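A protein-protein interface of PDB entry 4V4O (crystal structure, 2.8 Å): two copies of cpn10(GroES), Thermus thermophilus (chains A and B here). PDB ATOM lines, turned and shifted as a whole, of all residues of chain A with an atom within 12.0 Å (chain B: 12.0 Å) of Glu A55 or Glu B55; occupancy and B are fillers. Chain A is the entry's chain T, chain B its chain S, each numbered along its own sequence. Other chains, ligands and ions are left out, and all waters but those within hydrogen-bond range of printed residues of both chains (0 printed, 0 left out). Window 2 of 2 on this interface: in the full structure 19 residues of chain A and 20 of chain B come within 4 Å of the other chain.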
ATOM      1  N   ASP A  13      -4.724 -23.747  21.016  1.00  0.00           N
ATOM      2  CA  ASP A  13      -4.970 -23.298  19.642  1.00  0.00           C
ATOM      3  C   ASP A  13      -6.442 -23.257  19.234  1.00  0.00           C
ATOM      4  O   ASP A  13      -6.779 -23.120  18.052  1.00  0.00           O
ATOM      5  CB  ASP A  13      -4.130 -24.136  18.650  1.00  0.00           C
ATOM      6  CG  ASP A  13      -4.889 -25.307  18.026  1.00  0.00           C
ATOM      7  OD1 ASP A  13      -6.062 -25.551  18.375  1.00  0.00           O
ATOM      8  OD2 ASP A  13      -4.306 -25.997  17.167  1.00  0.00           O
ATOM      9  N   GLY A  51      -1.268 -20.688  21.842  1.00  0.00           N
ATOM     10  CA  GLY A  51      -1.013 -21.435  20.620  1.00  0.00           C
ATOM     11  C   GLY A  51      -0.942 -22.924  20.951  1.00  0.00           C
ATOM     12  O   GLY A  51      -1.237 -23.327  22.088  1.00  0.00           O
ATOM     13  N   ARG A  52      -0.555 -23.746  19.978  1.00  0.00           N
ATOM     14  CA  ARG A  52      -0.437 -25.189  20.203  1.00  0.00           C
ATOM     15  C   ARG A  52       0.970 -25.570  20.681  1.00  0.00           C
ATOM     16  O   ARG A  52       1.952 -25.375  19.960  1.00  0.00           O
ATOM     17  CB  ARG A  52      -0.741 -25.943  18.918  1.00  0.00           C
ATOM     18  CG  ARG A  52       0.303 -25.742  17.844  1.00  0.00           C
ATOM     19  CD  ARG A  52      -0.179 -26.255  16.513  1.00  0.00           C
ATOM     20  NE  ARG A  52       0.836 -26.125  15.473  1.00  0.00           N
ATOM     21  CZ  ARG A  52       1.322 -27.154  14.792  1.00  0.00           C
ATOM     22  NH1 ARG A  52       0.882 -28.368  15.054  1.00  0.00           N
ATOM     23  NH2 ARG A  52       2.234 -26.980  13.849  1.00  0.00           N
ATOM     24  N   VAL A  53       1.063 -26.119  21.892  1.00  0.00           N
ATOM     25  CA  VAL A  53       2.348 -26.530  22.475  1.00  0.00           C
ATOM     26  C   VAL A  53       3.074 -27.585  21.646  1.00  0.00           C
ATOM     27  O   VAL A  53       2.795 -28.784  21.756  1.00  0.00           O
ATOM     28  CB  VAL A  53       2.155 -27.078  23.901  1.00  0.00           C
ATOM     29  CG1 VAL A  53       3.434 -27.758  24.382  1.00  0.00           C
ATOM     30  CG2 VAL A  53       1.741 -25.941  24.836  1.00  0.00           C
ATOM     31  N   LEU A  54       4.025 -27.126  20.838  1.00  0.00           N
ATOM     32  CA  LEU A  54       4.803 -27.993  19.960  1.00  0.00           C
ATOM     33  C   LEU A  54       5.612 -29.060  20.699  1.00  0.00           C
ATOM     34  O   LEU A  54       5.575 -29.139  21.933  1.00  0.00           O
ATOM     35  CB  LEU A  54       5.721 -27.134  19.091  1.00  0.00           C
ATOM     36  CG  LEU A  54       6.191 -27.690  17.751  1.00  0.00           C
ATOM     37  CD1 LEU A  54       5.119 -28.502  17.076  1.00  0.00           C
ATOM     38  CD2 LEU A  54       6.564 -26.540  16.874  1.00  0.00           C
ATOM     39  N   GLU A  55       6.339 -29.873  19.929  1.00  0.00           N
ATOM     40  CA  GLU A  55       7.149 -30.976  20.457  1.00  0.00           C
ATOM     41  C   GLU A  55       8.315 -30.536  21.355  1.00  0.00           C
ATOM     42  O   GLU A  55       8.797 -31.314  22.181  1.00  0.00           O
ATOM     43  CB  GLU A  55       7.667 -31.818  19.289  1.00  0.00           C
ATOM     44  CG  GLU A  55       8.089 -33.210  19.668  1.00  0.00           C
ATOM     45  CD  GLU A  55       7.008 -34.223  19.467  1.00  0.00           C
ATOM     46  OE1 GLU A  55       5.862 -33.808  19.401  1.00  0.00           O
ATOM     47  OE2 GLU A  55       7.279 -35.432  19.382  1.00  0.00           O
ATOM     48  N   ASN A  56       8.772 -29.297  21.175  1.00  0.00           N
ATOM     49  CA  ASN A  56       9.855 -28.732  21.983  1.00  0.00           C
ATOM     50  C   ASN A  56       9.349 -27.454  22.648  1.00  0.00           C
ATOM     51  O   ASN A  56       9.703 -26.344  22.239  1.00  0.00           O
ATOM     52  CB  ASN A  56      11.083 -28.425  21.119  1.00  0.00           C
ATOM     53  CG  ASN A  56      10.724 -27.765  19.822  1.00  0.00           C
ATOM     54  OD1 ASN A  56       9.578 -27.442  19.604  1.00  0.00           O
ATOM     55  ND2 ASN A  56      11.701 -27.563  18.952  1.00  0.00           N
ATOM     56  N   GLY A  57       8.484 -27.640  23.648  1.00  0.00           N
ATOM     57  CA  GLY A  57       7.895 -26.553  24.420  1.00  0.00           C
ATOM     58  C   GLY A  57       7.467 -25.262  23.738  1.00  0.00           C
ATOM     59  O   GLY A  57       7.011 -24.353  24.421  1.00  0.00           O
ATOM     60  N   GLN A  58       7.587 -25.170  22.415  1.00  0.00           N
ATOM     61  CA  GLN A  58       7.217 -23.948  21.695  1.00  0.00           C
ATOM     62  C   GLN A  58       5.732 -23.805  21.336  1.00  0.00           C
ATOM     63  O   GLN A  58       5.180 -24.628  20.605  1.00  0.00           O
ATOM     64  CB  GLN A  58       8.020 -23.842  20.406  1.00  0.00           C
ATOM     65  CG  GLN A  58       9.509 -23.912  20.560  1.00  0.00           C
ATOM     66  CD  GLN A  58      10.190 -23.763  19.229  1.00  0.00           C
ATOM     67  OE1 GLN A  58       9.875 -24.475  18.300  1.00  0.00           O
ATOM     68  NE2 GLN A  58      11.120 -22.838  19.125  1.00  0.00           N
ATOM     69  N   ARG A  59       5.100 -22.740  21.820  1.00  0.00           N
ATOM     70  CA  ARG A  59       3.687 -22.495  21.542  1.00  0.00           C
ATOM     71  C   ARG A  59       3.466 -21.642  20.301  1.00  0.00           C
ATOM     72  O   ARG A  59       3.531 -20.414  20.360  1.00  0.00           O
ATOM     73  CB  ARG A  59       3.014 -21.816  22.736  1.00  0.00           C
ATOM     74  CG  ARG A  59       2.885 -22.702  23.957  1.00  0.00           C
ATOM     75  CD  ARG A  59       2.182 -21.978  25.090  1.00  0.00           C
ATOM     76  NE  ARG A  59       1.932 -22.860  26.227  1.00  0.00           N
ATOM     77  CZ  ARG A  59       1.352 -22.479  27.361  1.00  0.00           C
ATOM     78  NH1 ARG A  59       0.958 -21.223  27.520  1.00  0.00           N
ATOM     79  NH2 ARG A  59       1.169 -23.355  28.342  1.00  0.00           N
ATOM     80  N   VAL A  60       3.191 -22.304  19.181  1.00  0.00           N
ATOM     81  CA  VAL A  60       2.950 -21.615  17.917  1.00  0.00           C
ATOM     82  C   VAL A  60       1.664 -20.793  17.994  1.00  0.00           C
ATOM     83  O   VAL A  60       0.579 -21.341  18.194  1.00  0.00           O
ATOM     84  CB  VAL A  60       2.795 -22.616  16.743  1.00  0.00           C
ATOM     85  CG1 VAL A  60       2.833 -21.868  15.407  1.00  0.00           C
ATOM     86  CG2 VAL A  60       3.873 -23.695  16.815  1.00  0.00           C
ATOM     87  N   PRO A  61       1.769 -19.465  17.848  1.00  0.00           N
ATOM     88  CA  PRO A  61       0.566 -18.627  17.908  1.00  0.00           C
ATOM     89  C   PRO A  61      -0.383 -18.983  16.759  1.00  0.00           C
ATOM     90  O   PRO A  61       0.051 -19.477  15.713  1.00  0.00           O
ATOM     91  CB  PRO A  61       1.124 -17.209  17.775  1.00  0.00           C
ATOM     92  CG  PRO A  61       2.493 -17.325  18.355  1.00  0.00           C
ATOM     93  CD  PRO A  61       2.982 -18.635  17.789  1.00  0.00           C
ATOM     94  N   GLU A  92      -7.347 -25.365  15.159  1.00  0.00           N
ATOM     95  CA  GLU A  92      -6.608 -24.707  14.105  1.00  0.00           C
ATOM     96  C   GLU A  92      -6.816 -25.502  12.833  1.00  0.00           C
ATOM     97  O   GLU A  92      -6.912 -24.944  11.742  1.00  0.00           O
ATOM     98  CB  GLU A  92      -5.136 -24.678  14.495  1.00  0.00           C
ATOM     99  CG  GLU A  92      -4.230 -23.857  13.621  1.00  0.00           C
ATOM    100  CD  GLU A  92      -2.827 -23.815  14.187  1.00  0.00           C
ATOM    101  OE1 GLU A  92      -2.598 -24.444  15.238  1.00  0.00           O
ATOM    102  OE2 GLU A  92      -1.950 -23.161  13.594  1.00  0.00           O
ATOM    103  N   ARG A  93      -6.900 -26.816  12.997  1.00  0.00           N
ATOM    104  CA  ARG A  93      -7.089 -27.720  11.875  1.00  0.00           C
ATOM    105  C   ARG A  93      -8.361 -27.392  11.122  1.00  0.00           C
ATOM    106  O   ARG A  93      -8.370 -27.353   9.894  1.00  0.00           O
ATOM    107  CB  ARG A  93      -7.159 -29.153  12.378  1.00  0.00           C
ATOM    108  CG  ARG A  93      -5.958 -29.536  13.174  1.00  0.00           C
ATOM    109  CD  ARG A  93      -6.057 -30.954  13.624  1.00  0.00           C
ATOM    110  NE  ARG A  93      -4.842 -31.340  14.324  1.00  0.00           N
ATOM    111  CZ  ARG A  93      -4.788 -32.306  15.231  1.00  0.00           C
ATOM    112  NH1 ARG A  93      -5.885 -32.974  15.542  1.00  0.00           N
ATOM    113  NH2 ARG A  93      -3.640 -32.598  15.830  1.00  0.00           N
ATOM    114  N   ASP B  13      -2.957 -35.558  32.570  1.00  0.00           N
ATOM    115  CA  ASP B  13      -3.772 -34.566  31.873  1.00  0.00           C
ATOM    116  C   ASP B  13      -5.271 -34.570  32.240  1.00  0.00           C
ATOM    117  O   ASP B  13      -6.036 -33.700  31.817  1.00  0.00           O
ATOM    118  CB  ASP B  13      -3.487 -34.785  30.375  1.00  0.00           C
ATOM    119  CG  ASP B  13      -4.404 -34.065  29.462  1.00  0.00           C
ATOM    120  OD1 ASP B  13      -5.571 -33.845  29.806  1.00  0.00           O
ATOM    121  OD2 ASP B  13      -3.946 -33.756  28.348  1.00  0.00           O
ATOM    122  N   GLY B  51       0.873 -33.007  34.140  1.00  0.00           N
ATOM    123  CA  GLY B  51       0.611 -32.616  32.767  1.00  0.00           C
ATOM    124  C   GLY B  51       0.704 -33.846  31.867  1.00  0.00           C
ATOM    125  O   GLY B  51       0.943 -34.969  32.345  1.00  0.00           O
ATOM    126  N   ARG B  52       0.520 -33.649  30.565  1.00  0.00           N
ATOM    127  CA  ARG B  52       0.601 -34.771  29.632  1.00  0.00           C
ATOM    128  C   ARG B  52       2.017 -35.072  29.152  1.00  0.00           C
ATOM    129  O   ARG B  52       2.640 -34.236  28.504  1.00  0.00           O
ATOM    130  CB  ARG B  52      -0.256 -34.484  28.413  1.00  0.00           C
ATOM    131  CG  ARG B  52       0.254 -33.324  27.599  1.00  0.00           C
ATOM    132  CD  ARG B  52      -0.449 -33.302  26.276  1.00  0.00           C
ATOM    133  NE  ARG B  52       0.129 -32.306  25.389  1.00  0.00           N
ATOM    134  CZ  ARG B  52      -0.378 -31.988  24.206  1.00  0.00           C
ATOM    135  NH1 ARG B  52      -1.474 -32.593  23.779  1.00  0.00           N
ATOM    136  NH2 ARG B  52       0.208 -31.070  23.452  1.00  0.00           N
ATOM    137  N   VAL B  53       2.520 -36.265  29.445  1.00  0.00           N
ATOM    138  CA  VAL B  53       3.857 -36.654  29.026  1.00  0.00           C
ATOM    139  C   VAL B  53       3.987 -36.763  27.498  1.00  0.00           C
ATOM    140  O   VAL B  53       3.606 -37.771  26.918  1.00  0.00           O
ATOM    141  CB  VAL B  53       4.248 -38.020  29.662  1.00  0.00           C
ATOM    142  CG1 VAL B  53       5.643 -38.420  29.228  1.00  0.00           C
ATOM    143  CG2 VAL B  53       4.168 -37.935  31.176  1.00  0.00           C
ATOM    144  N   LEU B  54       4.498 -35.721  26.856  1.00  0.00           N
ATOM    145  CA  LEU B  54       4.690 -35.740  25.403  1.00  0.00           C
ATOM    146  C   LEU B  54       5.658 -36.845  24.964  1.00  0.00           C
ATOM    147  O   LEU B  54       5.990 -37.738  25.738  1.00  0.00           O
ATOM    148  CB  LEU B  54       5.292 -34.406  24.915  1.00  0.00           C
ATOM    149  CG  LEU B  54       4.362 -33.243  24.612  1.00  0.00           C
ATOM    150  CD1 LEU B  54       4.976 -32.328  23.622  1.00  0.00           C
ATOM    151  CD2 LEU B  54       3.148 -33.748  24.006  1.00  0.00           C
ATOM    152  N   GLU B  55       6.123 -36.746  23.719  1.00  0.00           N
ATOM    153  CA  GLU B  55       7.041 -37.717  23.136  1.00  0.00           C
ATOM    154  C   GLU B  55       8.492 -37.629  23.578  1.00  0.00           C
ATOM    155  O   GLU B  55       9.240 -38.617  23.449  1.00  0.00           O
ATOM    156  CB  GLU B  55       6.988 -37.607  21.624  1.00  0.00           C
ATOM    157  CG  GLU B  55       5.650 -37.970  21.065  1.00  0.00           C
ATOM    158  CD  GLU B  55       5.761 -38.376  19.628  1.00  0.00           C
ATOM    159  OE1 GLU B  55       6.835 -38.173  19.058  1.00  0.00           O
ATOM    160  OE2 GLU B  55       4.782 -38.895  19.057  1.00  0.00           O
ATOM    161  N   ASN B  56       8.935 -36.487  24.084  1.00  0.00           N
ATOM    162  CA  ASN B  56      10.299 -36.363  24.548  1.00  0.00           C
ATOM    163  C   ASN B  56      10.306 -36.278  26.066  1.00  0.00           C
ATOM    164  O   ASN B  56      11.160 -35.617  26.660  1.00  0.00           O
ATOM    165  CB  ASN B  56      10.993 -35.135  23.935  1.00  0.00           C
ATOM    166  CG  ASN B  56      10.019 -34.042  23.524  1.00  0.00           C
ATOM    167  OD1 ASN B  56       8.831 -34.162  23.763  1.00  0.00           O
ATOM    168  ND2 ASN B  56      10.515 -32.988  22.913  1.00  0.00           N
ATOM    169  N   GLY B  57       9.336 -36.946  26.686  1.00  0.00           N
ATOM    170  CA  GLY B  57       9.198 -36.975  28.119  1.00  0.00           C
ATOM    171  C   GLY B  57       8.833 -35.651  28.769  1.00  0.00           C
ATOM    172  O   GLY B  57       9.008 -35.484  29.983  1.00  0.00           O
ATOM    173  N   GLN B  58       8.323 -34.691  27.998  1.00  0.00           N
ATOM    174  CA  GLN B  58       8.012 -33.418  28.607  1.00  0.00           C
ATOM    175  C   GLN B  58       6.601 -33.116  29.022  1.00  0.00           C
ATOM    176  O   GLN B  58       5.761 -32.819  28.187  1.00  0.00           O
ATOM    177  CB  GLN B  58       8.545 -32.237  27.815  1.00  0.00           C
ATOM    178  CG  GLN B  58       8.549 -32.147  26.336  1.00  0.00           C
ATOM    179  CD  GLN B  58       9.225 -30.841  25.948  1.00  0.00           C
ATOM    180  OE1 GLN B  58       9.886 -30.215  26.772  1.00  0.00           O
ATOM    181  NE2 GLN B  58       9.064 -30.425  24.727  1.00  0.00           N
ATOM    182  N   ARG B  59       6.371 -33.135  30.338  1.00  0.00           N
ATOM    183  CA  ARG B  59       5.063 -32.894  30.921  1.00  0.00           C
ATOM    184  C   ARG B  59       4.556 -31.461  30.788  1.00  0.00           C
ATOM    185  O   ARG B  59       4.840 -30.604  31.625  1.00  0.00           O
ATOM    186  CB  ARG B  59       5.074 -33.330  32.396  1.00  0.00           C
ATOM    187  CG  ARG B  59       5.362 -34.815  32.586  1.00  0.00           C
ATOM    188  CD  ARG B  59       5.218 -35.251  34.041  1.00  0.00           C
ATOM    189  NE  ARG B  59       5.427 -36.691  34.202  1.00  0.00           N
ATOM    190  CZ  ARG B  59       5.346 -37.339  35.364  1.00  0.00           C
ATOM    191  NH1 ARG B  59       5.060 -36.676  36.475  1.00  0.00           N
ATOM    192  NH2 ARG B  59       5.550 -38.652  35.417  1.00  0.00           N
ATOM    193  N   VAL B  60       3.805 -31.214  29.718  1.00  0.00           N
ATOM    194  CA  VAL B  60       3.204 -29.908  29.474  1.00  0.00           C
ATOM    195  C   VAL B  60       2.047 -29.740  30.467  1.00  0.00           C
ATOM    196  O   VAL B  60       1.074 -30.506  30.457  1.00  0.00           O
ATOM    197  CB  VAL B  60       2.650 -29.821  28.047  1.00  0.00           C
ATOM    198  CG1 VAL B  60       2.177 -28.405  27.755  1.00  0.00           C
ATOM    199  CG2 VAL B  60       3.707 -30.261  27.059  1.00  0.00           C
ATOM    200  N   PRO B  61       2.141 -28.732  31.344  1.00  0.00           N
ATOM    201  CA  PRO B  61       1.111 -28.462  32.353  1.00  0.00           C
ATOM    202  C   PRO B  61      -0.243 -28.178  31.739  1.00  0.00           C
ATOM    203  O   PRO B  61      -0.337 -27.697  30.607  1.00  0.00           O
ATOM    204  CB  PRO B  61       1.657 -27.240  33.092  1.00  0.00           C
ATOM    205  CG  PRO B  61       3.125 -27.317  32.864  1.00  0.00           C
ATOM    206  CD  PRO B  61       3.225 -27.742  31.430  1.00  0.00           C
ATOM    207  N   GLU B  92      -7.725 -33.265  28.587  1.00  0.00           N
ATOM    208  CA  GLU B  92      -7.478 -31.943  28.053  1.00  0.00           C
ATOM    209  C   GLU B  92      -8.230 -31.762  26.745  1.00  0.00           C
ATOM    210  O   GLU B  92      -8.780 -30.691  26.480  1.00  0.00           O
ATOM    211  CB  GLU B  92      -5.979 -31.797  27.844  1.00  0.00           C
ATOM    212  CG  GLU B  92      -5.479 -30.453  27.418  1.00  0.00           C
ATOM    213  CD  GLU B  92      -3.966 -30.436  27.353  1.00  0.00           C
ATOM    214  OE1 GLU B  92      -3.352 -31.510  27.487  1.00  0.00           O
ATOM    215  OE2 GLU B  92      -3.381 -29.357  27.162  1.00  0.00           O
ATOM    216  N   ARG B  93      -8.262 -32.819  25.937  1.00  0.00           N
ATOM    217  CA  ARG B  93      -8.949 -32.771  24.655  1.00  0.00           C
ATOM    218  C   ARG B  93     -10.364 -32.265  24.868  1.00  0.00           C
ATOM    219  O   ARG B  93     -10.808 -31.325  24.215  1.00  0.00           O
ATOM    220  CB  ARG B  93      -9.013 -34.162  24.025  1.00  0.00           C
ATOM    221  CG  ARG B  93      -7.675 -34.842  23.829  1.00  0.00           C
ATOM    222  CD  ARG B  93      -7.836 -36.069  22.942  1.00  0.00           C
ATOM    223  NE  ARG B  93      -6.561 -36.717  22.648  1.00  0.00           N
ATOM    224  CZ  ARG B  93      -5.924 -37.532  23.481  1.00  0.00           C
ATOM    225  NH1 ARG B  93      -6.448 -37.808  24.664  1.00  0.00           N
ATOM    226  NH2 ARG B  93      -4.761 -38.065  23.135  1.00  0.00           N
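The backbone NH (N) of Arg B52 sits at hydrogen-bond distance from the backbone carbonyl oxygen (O) of Val B60, 3.2 Å away.
NE2 of Gln B58 sits close to ND2 of Asn B56, at 3.5 Å.
The side-chain amide oxygen of Asn A56 lies close to the side-chain amide oxygen of Gln A58, 3.3 Å away.
Val A53 touches Arg B52, but with the chains exchanged Arg A52 does not touch Val B53 (13.4 Å).
Glu B55 touches its own counterpart, Glu A55.
Glu A55 touches Asn B56, but with the chains exchanged Asn A56 does not touch Glu B55 (8.3 Å).
Asn A56 touches Gln B58, but with the chains exchanged Gln A58 does not touch Asn B56 (8.4 Å).
14 positions are printed for both chains.
Of the 8 pairs that touch across the chains among the printed residues, 2 have their exchanged pair printed and touching as well.
The backbone carbonyl oxygen (O) of Glu A55 is in hydrogen-bond range of the side-chain amide nitrogen (ND2) of Asn B56.
O of Glu A55 is in hydrogen-bond range of NE2 of Gln B58, 2.7 Å away.
The backbone NH (N) of Gly A57 lies close to the side-chain amide nitrogen (NE2) of Gln B58, 3.0 Å away.
OE1 of Glu B55 lies close to OE2 of Glu A55, 2.8 Å away.
Among the printed residues, merely in contact across the chains: Asn A56 with Gln B58 (3.3 Å), Val A53 with Val B60 (3.7 Å), Leu A54 with Leu B54 (3.7 Å) and Val A53 with Arg B52 (3.8 Å).
Printed residues of chain A that touch a printed residue of chain B: Val A53, Leu A54, Glu A55, Asn A56 and Gly A57.
Hydrophobic or aromatic side chains of chain B within 4 Å of the printed part of chain A: Leu B54 and Val B60.
Among the printed residues, no Asp or Glu carboxylate lies within 4 Å of a Lys or Arg side-chain nitrogen of the other chain.
Of chain B, only Glu B55 (2.8 Å), Asn B56 (2.5 Å) and Gln B58 (2.7 Å) come within 4 Å of Glu A55.
Glu B55 touches just one residue of chain A: Glu A55 (2.8 Å).
Of the printed residues of chain B, Val A53 touches Arg B52 and Val B60.
Leu A54 touches just one residue of chain B: Leu B54 (3.7 Å).
Gly A57 touches just one residue of chain B: Gln B58.
No residue of chain A comes within 4 Å of Val B53.
Leu B54 touches just one residue of chain A: Leu A54 (3.7 Å).
Gly B57 touches none of the printed residues of chain A.
Of chain A, only Glu A55, Asn A56 and Gly A57 come within 4 Å of Gln B58.
Of the printed residues of chain A, Arg B52 touches Val A53.
Printed residues of chain A within 4 Å of Val B60: Val A53.
Asp B13 touches none of the printed residues of chain A.
Pro A61 touches none of the printed residues of chain B.
The nearest residue of chain B that does not touch Glu A55 is Leu B54 (4.1 Å).
The nearest residue of chain A that does not touch Glu B55 is Leu A54 (7.8 Å).
The nearest printed residue of chain A that does not touch Val B60 is Arg A59 (5.2 Å).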
